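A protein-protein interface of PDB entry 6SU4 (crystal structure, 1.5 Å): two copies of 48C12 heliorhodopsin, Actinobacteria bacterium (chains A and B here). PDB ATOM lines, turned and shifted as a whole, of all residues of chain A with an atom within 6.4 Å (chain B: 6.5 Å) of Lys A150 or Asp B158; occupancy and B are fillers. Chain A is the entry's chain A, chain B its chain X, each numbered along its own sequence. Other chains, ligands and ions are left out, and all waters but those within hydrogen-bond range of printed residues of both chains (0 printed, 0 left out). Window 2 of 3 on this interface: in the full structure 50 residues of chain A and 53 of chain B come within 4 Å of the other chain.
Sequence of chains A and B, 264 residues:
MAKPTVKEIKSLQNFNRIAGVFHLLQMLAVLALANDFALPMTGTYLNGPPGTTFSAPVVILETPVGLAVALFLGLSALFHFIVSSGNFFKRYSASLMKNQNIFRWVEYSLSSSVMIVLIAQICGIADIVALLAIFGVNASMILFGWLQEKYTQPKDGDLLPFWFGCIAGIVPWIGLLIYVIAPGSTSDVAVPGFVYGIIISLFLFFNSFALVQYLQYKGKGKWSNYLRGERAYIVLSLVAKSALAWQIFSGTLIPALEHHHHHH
Of the 13 printed residues of chain A, 4 touch a printed residue of chain B. Printed residues of chain A that touch a printed residue of chain B: Trp A146, Lys A150, Tyr A151 and Thr A152. Hydrophobic or aromatic side chains of chain A that line the printed part of chain B: Trp A146 and Tyr A151. Along chain A the printed residues that touch a printed residue of chain B span positions 146 to 152. Printed residues of chain B that touch a printed residue of chain A: Tyr B151, Thr B152, Asp B158, Leu B160 and Pro B161. Hydrophobic or aromatic side chains of chain B within 4 Å of the printed part of chain A: Tyr B151, Leu B160 and Pro B161. Among the printed residues, 8 pairs touch across the chains. Among the printed residues, no Asp or Glu carboxylate lies within 4 Å of a Lys or Arg side-chain nitrogen of the other chain.
Of chain B, only Asp B158 (3.8 Å) and Leu B160 (3.6 Å) come within 4 Å of Lys A150. Of the printed residues of chain B, Tyr A151 touches Tyr B151 (3.4 Å), Thr B152 (3.9 Å), Asp B158 (2.6 Å) and Pro B161 (3.3 Å). Printed residues of chain A within 4 Å of Tyr B151: Tyr A151 and Thr A152. The nearest residue of chain B that does not touch Lys A150 is Pro B161 (5.7 Å). The nearest printed residue of chain A that does not touch Pro B161 is Leu A147 (4.1 Å).
The backbone carbonyl oxygen (O) of Gln B148 is in hydrogen-bond range of the side-chain hydroxyl (OG1) of Thr B152 (2.6 Å). NE2 of Gln B148 sits at hydrogen-bond distance from O of Asp B158, at 2.9 Å. OD1 of Asp B156 is in hydrogen-bond range of N of Asp B158 (2.7 Å). N of Leu B160 lies within hydrogen-bond range of OD1 of Asp B158 (3.2 Å). The side-chain hydroxyl of Thr A152 lies within hydrogen-bond range of the backbone carbonyl oxygen of Gln A148 (2.7 Å).
The side-chain hydroxyl (OH) of Tyr A151 sits at hydrogen-bond distance from the side-chain carboxylate (OD2) of Asp B158 (2.6 Å).
Tyr A151 touches its own counterpart, Tyr B151. Tyr A151 touches Thr B152, and with the chains exchanged Thr A152 touches Tyr B151. Positions printed for both chains: 148, 151, 152, 153 and 217. Of the 8 pairs that touch across the chains among the printed residues, 3 have their exchanged pair printed and touching as well.
Among the printed residues, merely in contact across the chains: Trp A146 with Leu B160 (3.6 Å), Lys A150 with Asp B158 (3.8 Å), Lys A150 with Leu B160 (3.6 Å), Tyr A151 with Tyr B151 (3.4 Å), Tyr A151 with Thr B152 (3.9 Å), Tyr A151 with Pro B161 (3.3 Å) and Thr A152 with Tyr B151 (3.8 Å).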
ATOM      1  N   ASN A  99      -5.914   9.375  23.700  1.00  0.00           N
ATOM      2  CA  ASN A  99      -6.250  10.742  24.175  1.00  0.00           C
ATOM      3  C   ASN A  99      -5.602  11.771  23.234  1.00  0.00           C
ATOM      4  O   ASN A  99      -5.026  12.753  23.727  1.00  0.00           O
ATOM      5  CB  ASN A  99      -5.811  10.945  25.628  1.00  0.00           C
ATOM      6  CG  ASN A  99      -6.363   9.877  26.548  1.00  0.00           C
ATOM      7  OD1 ASN A  99      -7.524   9.491  26.427  1.00  0.00           O
ATOM      8  ND2 ASN A  99      -5.541   9.385  27.458  1.00  0.00           N
ATOM      9  N   GLN A 100      -5.707  11.558  21.921  1.00  0.00           N
ATOM     10  CA  GLN A 100      -5.136  12.469  20.896  1.00  0.00           C
ATOM     11  C   GLN A 100      -6.125  12.654  19.744  1.00  0.00           C
ATOM     12  O   GLN A 100      -6.850  11.699  19.414  1.00  0.00           O
ATOM     13  CB  GLN A 100      -3.835  11.917  20.322  1.00  0.00           C
ATOM     14  CG  GLN A 100      -2.705  11.814  21.337  1.00  0.00           C
ATOM     15  CD  GLN A 100      -1.476  11.234  20.687  1.00  0.00           C
ATOM     16  OE1 GLN A 100      -1.346  11.244  19.468  1.00  0.00           O
ATOM     17  NE2 GLN A 100      -0.564  10.724  21.497  1.00  0.00           N
ATOM     18  N   ILE A 102      -4.996  14.527  16.279  1.00  0.00           N
ATOM     19  CA  ILE A 102      -4.010  15.318  15.488  1.00  0.00           C
ATOM     20  C   ILE A 102      -4.740  16.127  14.403  1.00  0.00           C
ATOM     21  O   ILE A 102      -4.369  17.279  14.162  1.00  0.00           O
ATOM     22  CB  ILE A 102      -2.903  14.413  14.917  1.00  0.00           C
ATOM     23  CG1 ILE A 102      -2.150  13.671  16.026  1.00  0.00           C
ATOM     24  CG2 ILE A 102      -1.961  15.211  14.033  1.00  0.00           C
ATOM     25  CD1 ILE A 102      -2.267  14.313  17.387  1.00  0.00           C
ATOM     26  N   GLY A 145      -0.921  22.928  22.277  1.00  0.00           N
ATOM     27  CA  GLY A 145      -2.045  22.049  22.648  1.00  0.00           C
ATOM     28  C   GLY A 145      -1.841  20.641  22.113  1.00  0.00           C
ATOM     29  O   GLY A 145      -2.168  19.666  22.813  1.00  0.00           O
ATOM     30  N   TRP A 146      -1.344  20.528  20.886  1.00  0.00           N
ATOM     31  CA  TRP A 146      -0.987  19.230  20.259  1.00  0.00           C
ATOM     32  C   TRP A 146       0.096  18.539  21.102  1.00  0.00           C
ATOM     33  O   TRP A 146      -0.055  17.342  21.405  1.00  0.00           O
ATOM     34  CB  TRP A 146      -0.562  19.522  18.818  1.00  0.00           C
ATOM     35  CG  TRP A 146      -0.052  18.396  17.979  1.00  0.00           C
ATOM     36  CD1 TRP A 146       0.447  17.178  18.343  1.00  0.00           C
ATOM     37  CD2 TRP A 146       0.088  18.472  16.553  1.00  0.00           C
ATOM     38  NE1 TRP A 146       0.869  16.486  17.234  1.00  0.00           N
ATOM     39  CE2 TRP A 146       0.669  17.262  16.123  1.00  0.00           C
ATOM     40  CE3 TRP A 146      -0.210  19.464  15.613  1.00  0.00           C
ATOM     41  CZ2 TRP A 146       0.933  17.013  14.777  1.00  0.00           C
ATOM     42  CZ3 TRP A 146       0.050  19.212  14.284  1.00  0.00           C
ATOM     43  CH2 TRP A 146       0.615  18.004  13.877  1.00  0.00           C
ATOM     44  N   LEU A 147       1.128  19.266  21.535  1.00  0.00           N
ATOM     45  CA  LEU A 147       2.232  18.669  22.319  1.00  0.00           C
ATOM     46  C   LEU A 147       1.729  18.241  23.705  1.00  0.00           C
ATOM     47  O   LEU A 147       2.222  17.223  24.215  1.00  0.00           O
ATOM     48  CB  LEU A 147       3.406  19.650  22.394  1.00  0.00           C
ATOM     49  CG  LEU A 147       4.070  19.955  21.054  1.00  0.00           C
ATOM     50  CD1 LEU A 147       5.322  20.780  21.257  1.00  0.00           C
ATOM     51  CD2 LEU A 147       4.382  18.678  20.286  1.00  0.00           C
ATOM     52  N   GLN A 148       0.777  18.964  24.292  1.00  0.00           N
ATOM     53  CA  GLN A 148       0.139  18.548  25.572  1.00  0.00           C
ATOM     54  C   GLN A 148      -0.433  17.138  25.391  1.00  0.00           C
ATOM     55  O   GLN A 148      -0.180  16.254  26.246  1.00  0.00           O
ATOM     56  CB  GLN A 148      -0.928  19.558  25.991  1.00  0.00           C
ATOM     57  CG  GLN A 148      -1.661  19.178  27.275  1.00  0.00           C
ATOM     58  CD  GLN A 148      -0.824  19.375  28.516  1.00  0.00           C
ATOM     59  OE1 GLN A 148      -0.045  20.317  28.621  1.00  0.00           O
ATOM     60  NE2 GLN A 148      -0.998  18.498  29.495  1.00  0.00           N
ATOM     61  N   GLU A 149      -1.226  16.933  24.337  1.00  0.00           N
ATOM     62  CA  GLU A 149      -1.824  15.602  24.037  1.00  0.00           C
ATOM     63  C   GLU A 149      -0.742  14.571  23.703  1.00  0.00           C
ATOM     64  O   GLU A 149      -0.907  13.390  24.073  1.00  0.00           O
ATOM     65  CB  GLU A 149      -2.802  15.694  22.870  1.00  0.00           C
ATOM     66  CG  GLU A 149      -4.076  16.413  23.228  1.00  0.00           C
ATOM     67  CD  GLU A 149      -5.212  16.153  22.259  1.00  0.00           C
ATOM     68  OE1 GLU A 149      -4.929  15.755  21.102  1.00  0.00           O
ATOM     69  OE2 GLU A 149      -6.357  16.346  22.664  1.00  0.00           O
ATOM     70  N   LYS A 150       0.310  14.963  22.990  1.00  0.00           N
ATOM     71  CA  LYS A 150       1.304  13.984  22.488  1.00  0.00           C
ATOM     72  C   LYS A 150       2.111  13.433  23.666  1.00  0.00           C
ATOM     73  O   LYS A 150       2.359  12.222  23.692  1.00  0.00           O
ATOM     74  CB  LYS A 150       2.215  14.618  21.435  1.00  0.00           C
ATOM     75  CG  LYS A 150       3.209  13.660  20.799  1.00  0.00           C
ATOM     76  CD  LYS A 150       4.106  14.325  19.779  1.00  0.00           C
ATOM     77  CE  LYS A 150       5.105  13.375  19.158  1.00  0.00           C
ATOM     78  NZ  LYS A 150       4.443  12.482  18.186  1.00  0.00           N
ATOM     79  N   TYR A 151       2.524  14.278  24.610  1.00  0.00           N
ATOM     80  CA  TYR A 151       3.599  13.913  25.563  1.00  0.00           C
ATOM     81  C   TYR A 151       3.086  13.676  26.981  1.00  0.00           C
ATOM     82  O   TYR A 151       3.847  13.068  27.762  1.00  0.00           O
ATOM     83  CB  TYR A 151       4.693  14.973  25.544  1.00  0.00           C
ATOM     84  CG  TYR A 151       5.454  14.985  24.248  1.00  0.00           C
ATOM     85  CD1 TYR A 151       6.047  13.835  23.756  1.00  0.00           C
ATOM     86  CD2 TYR A 151       5.567  16.144  23.501  1.00  0.00           C
ATOM     87  CE1 TYR A 151       6.756  13.838  22.566  1.00  0.00           C
ATOM     88  CE2 TYR A 151       6.254  16.160  22.303  1.00  0.00           C
ATOM     89  CZ  TYR A 151       6.855  15.007  21.834  1.00  0.00           C
ATOM     90  OH  TYR A 151       7.538  15.033  20.650  1.00  0.00           O
ATOM     91  N   THR A 152       1.891  14.148  27.335  1.00  0.00           N
ATOM     92  CA  THR A 152       1.400  14.043  28.734  1.00  0.00           C
ATOM     93  C   THR A 152       0.210  13.092  28.790  1.00  0.00           C
ATOM     94  O   THR A 152      -0.373  12.801  27.739  1.00  0.00           O
ATOM     95  CB  THR A 152       1.030  15.404  29.337  1.00  0.00           C
ATOM     96  OG1 THR A 152      -0.269  15.771  28.867  1.00  0.00           O
ATOM     97  CG2 THR A 152       2.057  16.470  29.025  1.00  0.00           C
ATOM     98  N   GLN A 153      -0.130  12.662  30.002  1.00  0.00           N
ATOM     99  CA  GLN A 153      -1.344  11.868  30.306  1.00  0.00           C
ATOM    100  C   GLN A 153      -2.236  12.698  31.211  1.00  0.00           C
ATOM    101  O   GLN A 153      -1.744  13.360  32.120  1.00  0.00           O
ATOM    102  CB  GLN A 153      -0.981  10.580  31.047  1.00  0.00           C
ATOM    103  CG  GLN A 153       0.147   9.803  30.394  1.00  0.00           C
ATOM    104  CD  GLN A 153      -0.256   9.379  29.008  1.00  0.00           C
ATOM    105  OE1 GLN A 153      -1.440   9.269  28.709  1.00  0.00           O
ATOM    106  NE2 GLN A 153       0.731   9.163  28.151  1.00  0.00           N
ATOM    107  N   TYR A 217      -7.006  17.374  31.197  1.00  0.00           N
ATOM    108  CA  TYR A 217      -5.672  16.990  31.724  1.00  0.00           C
ATOM    109  C   TYR A 217      -5.646  17.123  33.248  1.00  0.00           C
ATOM    110  O   TYR A 217      -4.826  16.422  33.859  1.00  0.00           O
ATOM    111  CB  TYR A 217      -4.563  17.669  30.912  1.00  0.00           C
ATOM    112  CG  TYR A 217      -4.387  16.937  29.612  1.00  0.00           C
ATOM    113  CD1 TYR A 217      -5.246  17.185  28.555  1.00  0.00           C
ATOM    114  CD2 TYR A 217      -3.494  15.883  29.493  1.00  0.00           C
ATOM    115  CE1 TYR A 217      -5.185  16.445  27.389  1.00  0.00           C
ATOM    116  CE2 TYR A 217      -3.407  15.142  28.326  1.00  0.00           C
ATOM    117  CZ  TYR A 217      -4.261  15.422  27.272  1.00  0.00           C
ATOM    118  OH  TYR A 217      -4.226  14.682  26.124  1.00  0.00           O
ATOM    119  N   GLN B 148      11.151  20.117  23.267  1.00  0.00           N
ATOM    120  CA  GLN B 148      12.011  19.098  22.613  1.00  0.00           C
ATOM    121  C   GLN B 148      12.891  18.442  23.685  1.00  0.00           C
ATOM    122  O   GLN B 148      12.932  17.200  23.733  1.00  0.00           O
ATOM    123  CB  GLN B 148      12.843  19.727  21.493  1.00  0.00           C
ATOM    124  CG  GLN B 148      13.792  18.747  20.816  1.00  0.00           C
ATOM    125  CD  GLN B 148      13.099  17.775  19.890  1.00  0.00           C
ATOM    126  OE1 GLN B 148      12.130  18.108  19.207  1.00  0.00           O
ATOM    127  NE2 GLN B 148      13.624  16.556  19.835  1.00  0.00           N
ATOM    128  N   TYR B 151      10.696  16.347  26.564  1.00  0.00           N
ATOM    129  CA  TYR B 151       9.882  15.147  26.234  1.00  0.00           C
ATOM    130  C   TYR B 151      10.599  14.144  25.327  1.00  0.00           C
ATOM    131  O   TYR B 151      10.069  13.025  25.205  1.00  0.00           O
ATOM    132  CB  TYR B 151       8.551  15.569  25.617  1.00  0.00           C
ATOM    133  CG  TYR B 151       7.673  16.324  26.579  1.00  0.00           C
ATOM    134  CD1 TYR B 151       7.304  15.779  27.799  1.00  0.00           C
ATOM    135  CD2 TYR B 151       7.224  17.594  26.273  1.00  0.00           C
ATOM    136  CE1 TYR B 151       6.492  16.469  28.686  1.00  0.00           C
ATOM    137  CE2 TYR B 151       6.411  18.295  27.144  1.00  0.00           C
ATOM    138  CZ  TYR B 151       6.041  17.734  28.353  1.00  0.00           C
ATOM    139  OH  TYR B 151       5.253  18.453  29.205  1.00  0.00           O
ATOM    140  N   THR B 152      11.718  14.500  24.701  1.00  0.00           N
ATOM    141  CA  THR B 152      12.471  13.567  23.817  1.00  0.00           C
ATOM    142  C   THR B 152      13.874  13.340  24.385  1.00  0.00           C
ATOM    143  O   THR B 152      14.305  14.107  25.266  1.00  0.00           O
ATOM    144  CB  THR B 152      12.509  14.080  22.370  1.00  0.00           C
ATOM    145  OG1 THR B 152      13.534  15.069  22.296  1.00  0.00           O
ATOM    146  CG2 THR B 152      11.180  14.625  21.892  1.00  0.00           C
ATOM    147  N   GLN B 153      14.583  12.345  23.856  1.00  0.00           N
ATOM    148  CA  GLN B 153      16.038  12.180  24.078  1.00  0.00           C
ATOM    149  C   GLN B 153      16.708  12.065  22.716  1.00  0.00           C
ATOM    150  O   GLN B 153      16.094  11.622  21.751  1.00  0.00           O
ATOM    151  CB  GLN B 153      16.359  10.950  24.936  1.00  0.00           C
ATOM    152  CG  GLN B 153      15.841  11.049  26.366  1.00  0.00           C
ATOM    153  CD  GLN B 153      16.454  12.177  27.160  1.00  0.00           C
ATOM    154  OE1 GLN B 153      17.500  12.722  26.814  1.00  0.00           O
ATOM    155  NE2 GLN B 153      15.801  12.537  28.253  1.00  0.00           N
ATOM    156  N   LYS B 155      18.446  10.742  19.519  1.00  0.00           N
ATOM    157  CA  LYS B 155      18.514   9.462  18.765  1.00  0.00           C
ATOM    158  C   LYS B 155      17.214   8.663  18.927  1.00  0.00           C
ATOM    159  O   LYS B 155      17.204   7.494  18.504  1.00  0.00           O
ATOM    160  CB  LYS B 155      19.711   8.626  19.233  1.00  0.00           C
ATOM    161  CG  LYS B 155      21.074   9.284  19.063  1.00  0.00           C
ATOM    162  CD  LYS B 155      22.230   8.303  19.095  1.00  0.00           C
ATOM    163  N   ASP B 156      16.154   9.265  19.481  1.00  0.00           N
ATOM    164  CA  ASP B 156      14.848   8.580  19.693  1.00  0.00           C
ATOM    165  C   ASP B 156      13.955   8.784  18.464  1.00  0.00           C
ATOM    166  O   ASP B 156      12.852   8.224  18.445  1.00  0.00           O
ATOM    167  CB  ASP B 156      14.186   9.017  21.004  1.00  0.00           C
ATOM    168  CG  ASP B 156      13.352  10.290  20.920  1.00  0.00           C
ATOM    169  OD1 ASP B 156      13.291  10.892  19.818  1.00  0.00           O
ATOM    170  OD2 ASP B 156      12.765  10.671  21.966  1.00  0.00           O
ATOM    171  N   GLY B 157      14.418   9.555  17.473  1.00  0.00           N
ATOM    172  CA  GLY B 157      13.752   9.719  16.165  1.00  0.00           C
ATOM    173  C   GLY B 157      12.634  10.756  16.179  1.00  0.00           C
ATOM    174  O   GLY B 157      11.949  10.894  15.160  1.00  0.00           O
ATOM    175  N   ASP B 158      12.462  11.491  17.278  1.00  0.00           N
ATOM    176  CA  ASP B 158      11.321  12.423  17.463  1.00  0.00           C
ATOM    177  C   ASP B 158      11.830  13.871  17.462  1.00  0.00           C
ATOM    178  O   ASP B 158      12.523  14.251  18.420  1.00  0.00           O
ATOM    179  CB  ASP B 158      10.580  12.097  18.759  1.00  0.00           C
ATOM    180  CG  ASP B 158       9.344  12.942  18.998  1.00  0.00           C
ATOM    181  OD1 ASP B 158       8.968  13.716  18.086  1.00  0.00           O
ATOM    182  OD2 ASP B 158       8.770  12.817  20.092  1.00  0.00           O
ATOM    183  N   LEU B 159      11.525  14.623  16.403  1.00  0.00           N
ATOM    184  CA  LEU B 159      11.896  16.060  16.278  1.00  0.00           C
ATOM    185  C   LEU B 159      10.633  16.928  16.177  1.00  0.00           C
ATOM    186  O   LEU B 159      10.742  18.054  15.675  1.00  0.00           O
ATOM    187  CB  LEU B 159      12.771  16.253  15.034  1.00  0.00           C
ATOM    188  CG  LEU B 159      14.204  15.734  15.142  1.00  0.00           C
ATOM    189  CD1 LEU B 159      14.906  15.824  13.796  1.00  0.00           C
ATOM    190  CD2 LEU B 159      14.984  16.500  16.197  1.00  0.00           C
ATOM    191  N   LEU B 160       9.463  16.462  16.616  1.00  0.00           N
ATOM    192  CA  LEU B 160       8.223  17.240  16.359  1.00  0.00           C
ATOM    193  C   LEU B 160       8.317  18.614  17.024  1.00  0.00           C
ATOM    194  O   LEU B 160       8.040  19.619  16.374  1.00  0.00           O
ATOM    195  CB  LEU B 160       6.970  16.500  16.834  1.00  0.00           C
ATOM    196  CG  LEU B 160       5.670  17.149  16.361  1.00  0.00           C
ATOM    197  CD1 LEU B 160       5.619  17.225  14.841  1.00  0.00           C
ATOM    198  CD2 LEU B 160       4.455  16.417  16.910  1.00  0.00           C
ATOM    199  N   PRO B 161       8.672  18.726  18.326  1.00  0.00           N
ATOM    200  CA  PRO B 161       8.730  20.044  18.969  1.00  0.00           C
ATOM    201  C   PRO B 161       9.727  20.954  18.235  1.00  0.00           C
ATOM    202  O   PRO B 161       9.445  22.132  18.008  1.00  0.00           O
ATOM    203  CB  PRO B 161       9.164  19.725  20.405  1.00  0.00           C
ATOM    204  CG  PRO B 161       8.681  18.302  20.607  1.00  0.00           C
ATOM    205  CD  PRO B 161       8.951  17.633  19.272  1.00  0.00           C
ATOM    206  N   PHE B 162      10.863  20.386  17.838  1.00  0.00           N
ATOM    207  CA  PHE B 162      11.915  21.115  17.092  1.00  0.00           C
ATOM    208  C   PHE B 162      11.308  21.728  15.826  1.00  0.00           C
ATOM    209  O   PHE B 162      11.514  22.927  15.536  1.00  0.00           O
ATOM    210  CB  PHE B 162      13.094  20.203  16.745  1.00  0.00           C
ATOM    211  CG  PHE B 162      14.066  20.862  15.805  1.00  0.00           C
ATOM    212  CD1 PHE B 162      14.995  21.773  16.283  1.00  0.00           C
ATOM    213  CD2 PHE B 162      14.012  20.618  14.444  1.00  0.00           C
ATOM    214  CE1 PHE B 162      15.877  22.398  15.419  1.00  0.00           C
ATOM    215  CE2 PHE B 162      14.904  21.239  13.582  1.00  0.00           C
ATOM    216  CZ  PHE B 162      15.830  22.127  14.072  1.00  0.00           C
ATOM    217  N   TYR B 217      19.982  16.228  18.777  1.00  0.00           N
ATOM    218  CA  TYR B 217      18.859  15.252  18.865  1.00  0.00           C
ATOM    219  C   TYR B 217      18.956  14.224  17.730  1.00  0.00           C
ATOM    220  O   TYR B 217      18.416  13.110  17.888  1.00  0.00           O
ATOM    221  CB  TYR B 217      17.524  15.989  19.043  1.00  0.00           C
ATOM    222  CG  TYR B 217      17.362  16.382  20.486  1.00  0.00           C
ATOM    223  CD1 TYR B 217      16.675  15.571  21.377  1.00  0.00           C
ATOM    224  CD2 TYR B 217      18.036  17.474  21.001  1.00  0.00           C
ATOM    225  CE1 TYR B 217      16.600  15.881  22.724  1.00  0.00           C
ATOM    226  CE2 TYR B 217      17.991  17.785  22.348  1.00  0.00           C
ATOM    227  CZ  TYR B 217      17.274  16.980  23.216  1.00  0.00           C
ATOM    228  OH  TYR B 217      17.232  17.294  24.541  1.00  0.00           O
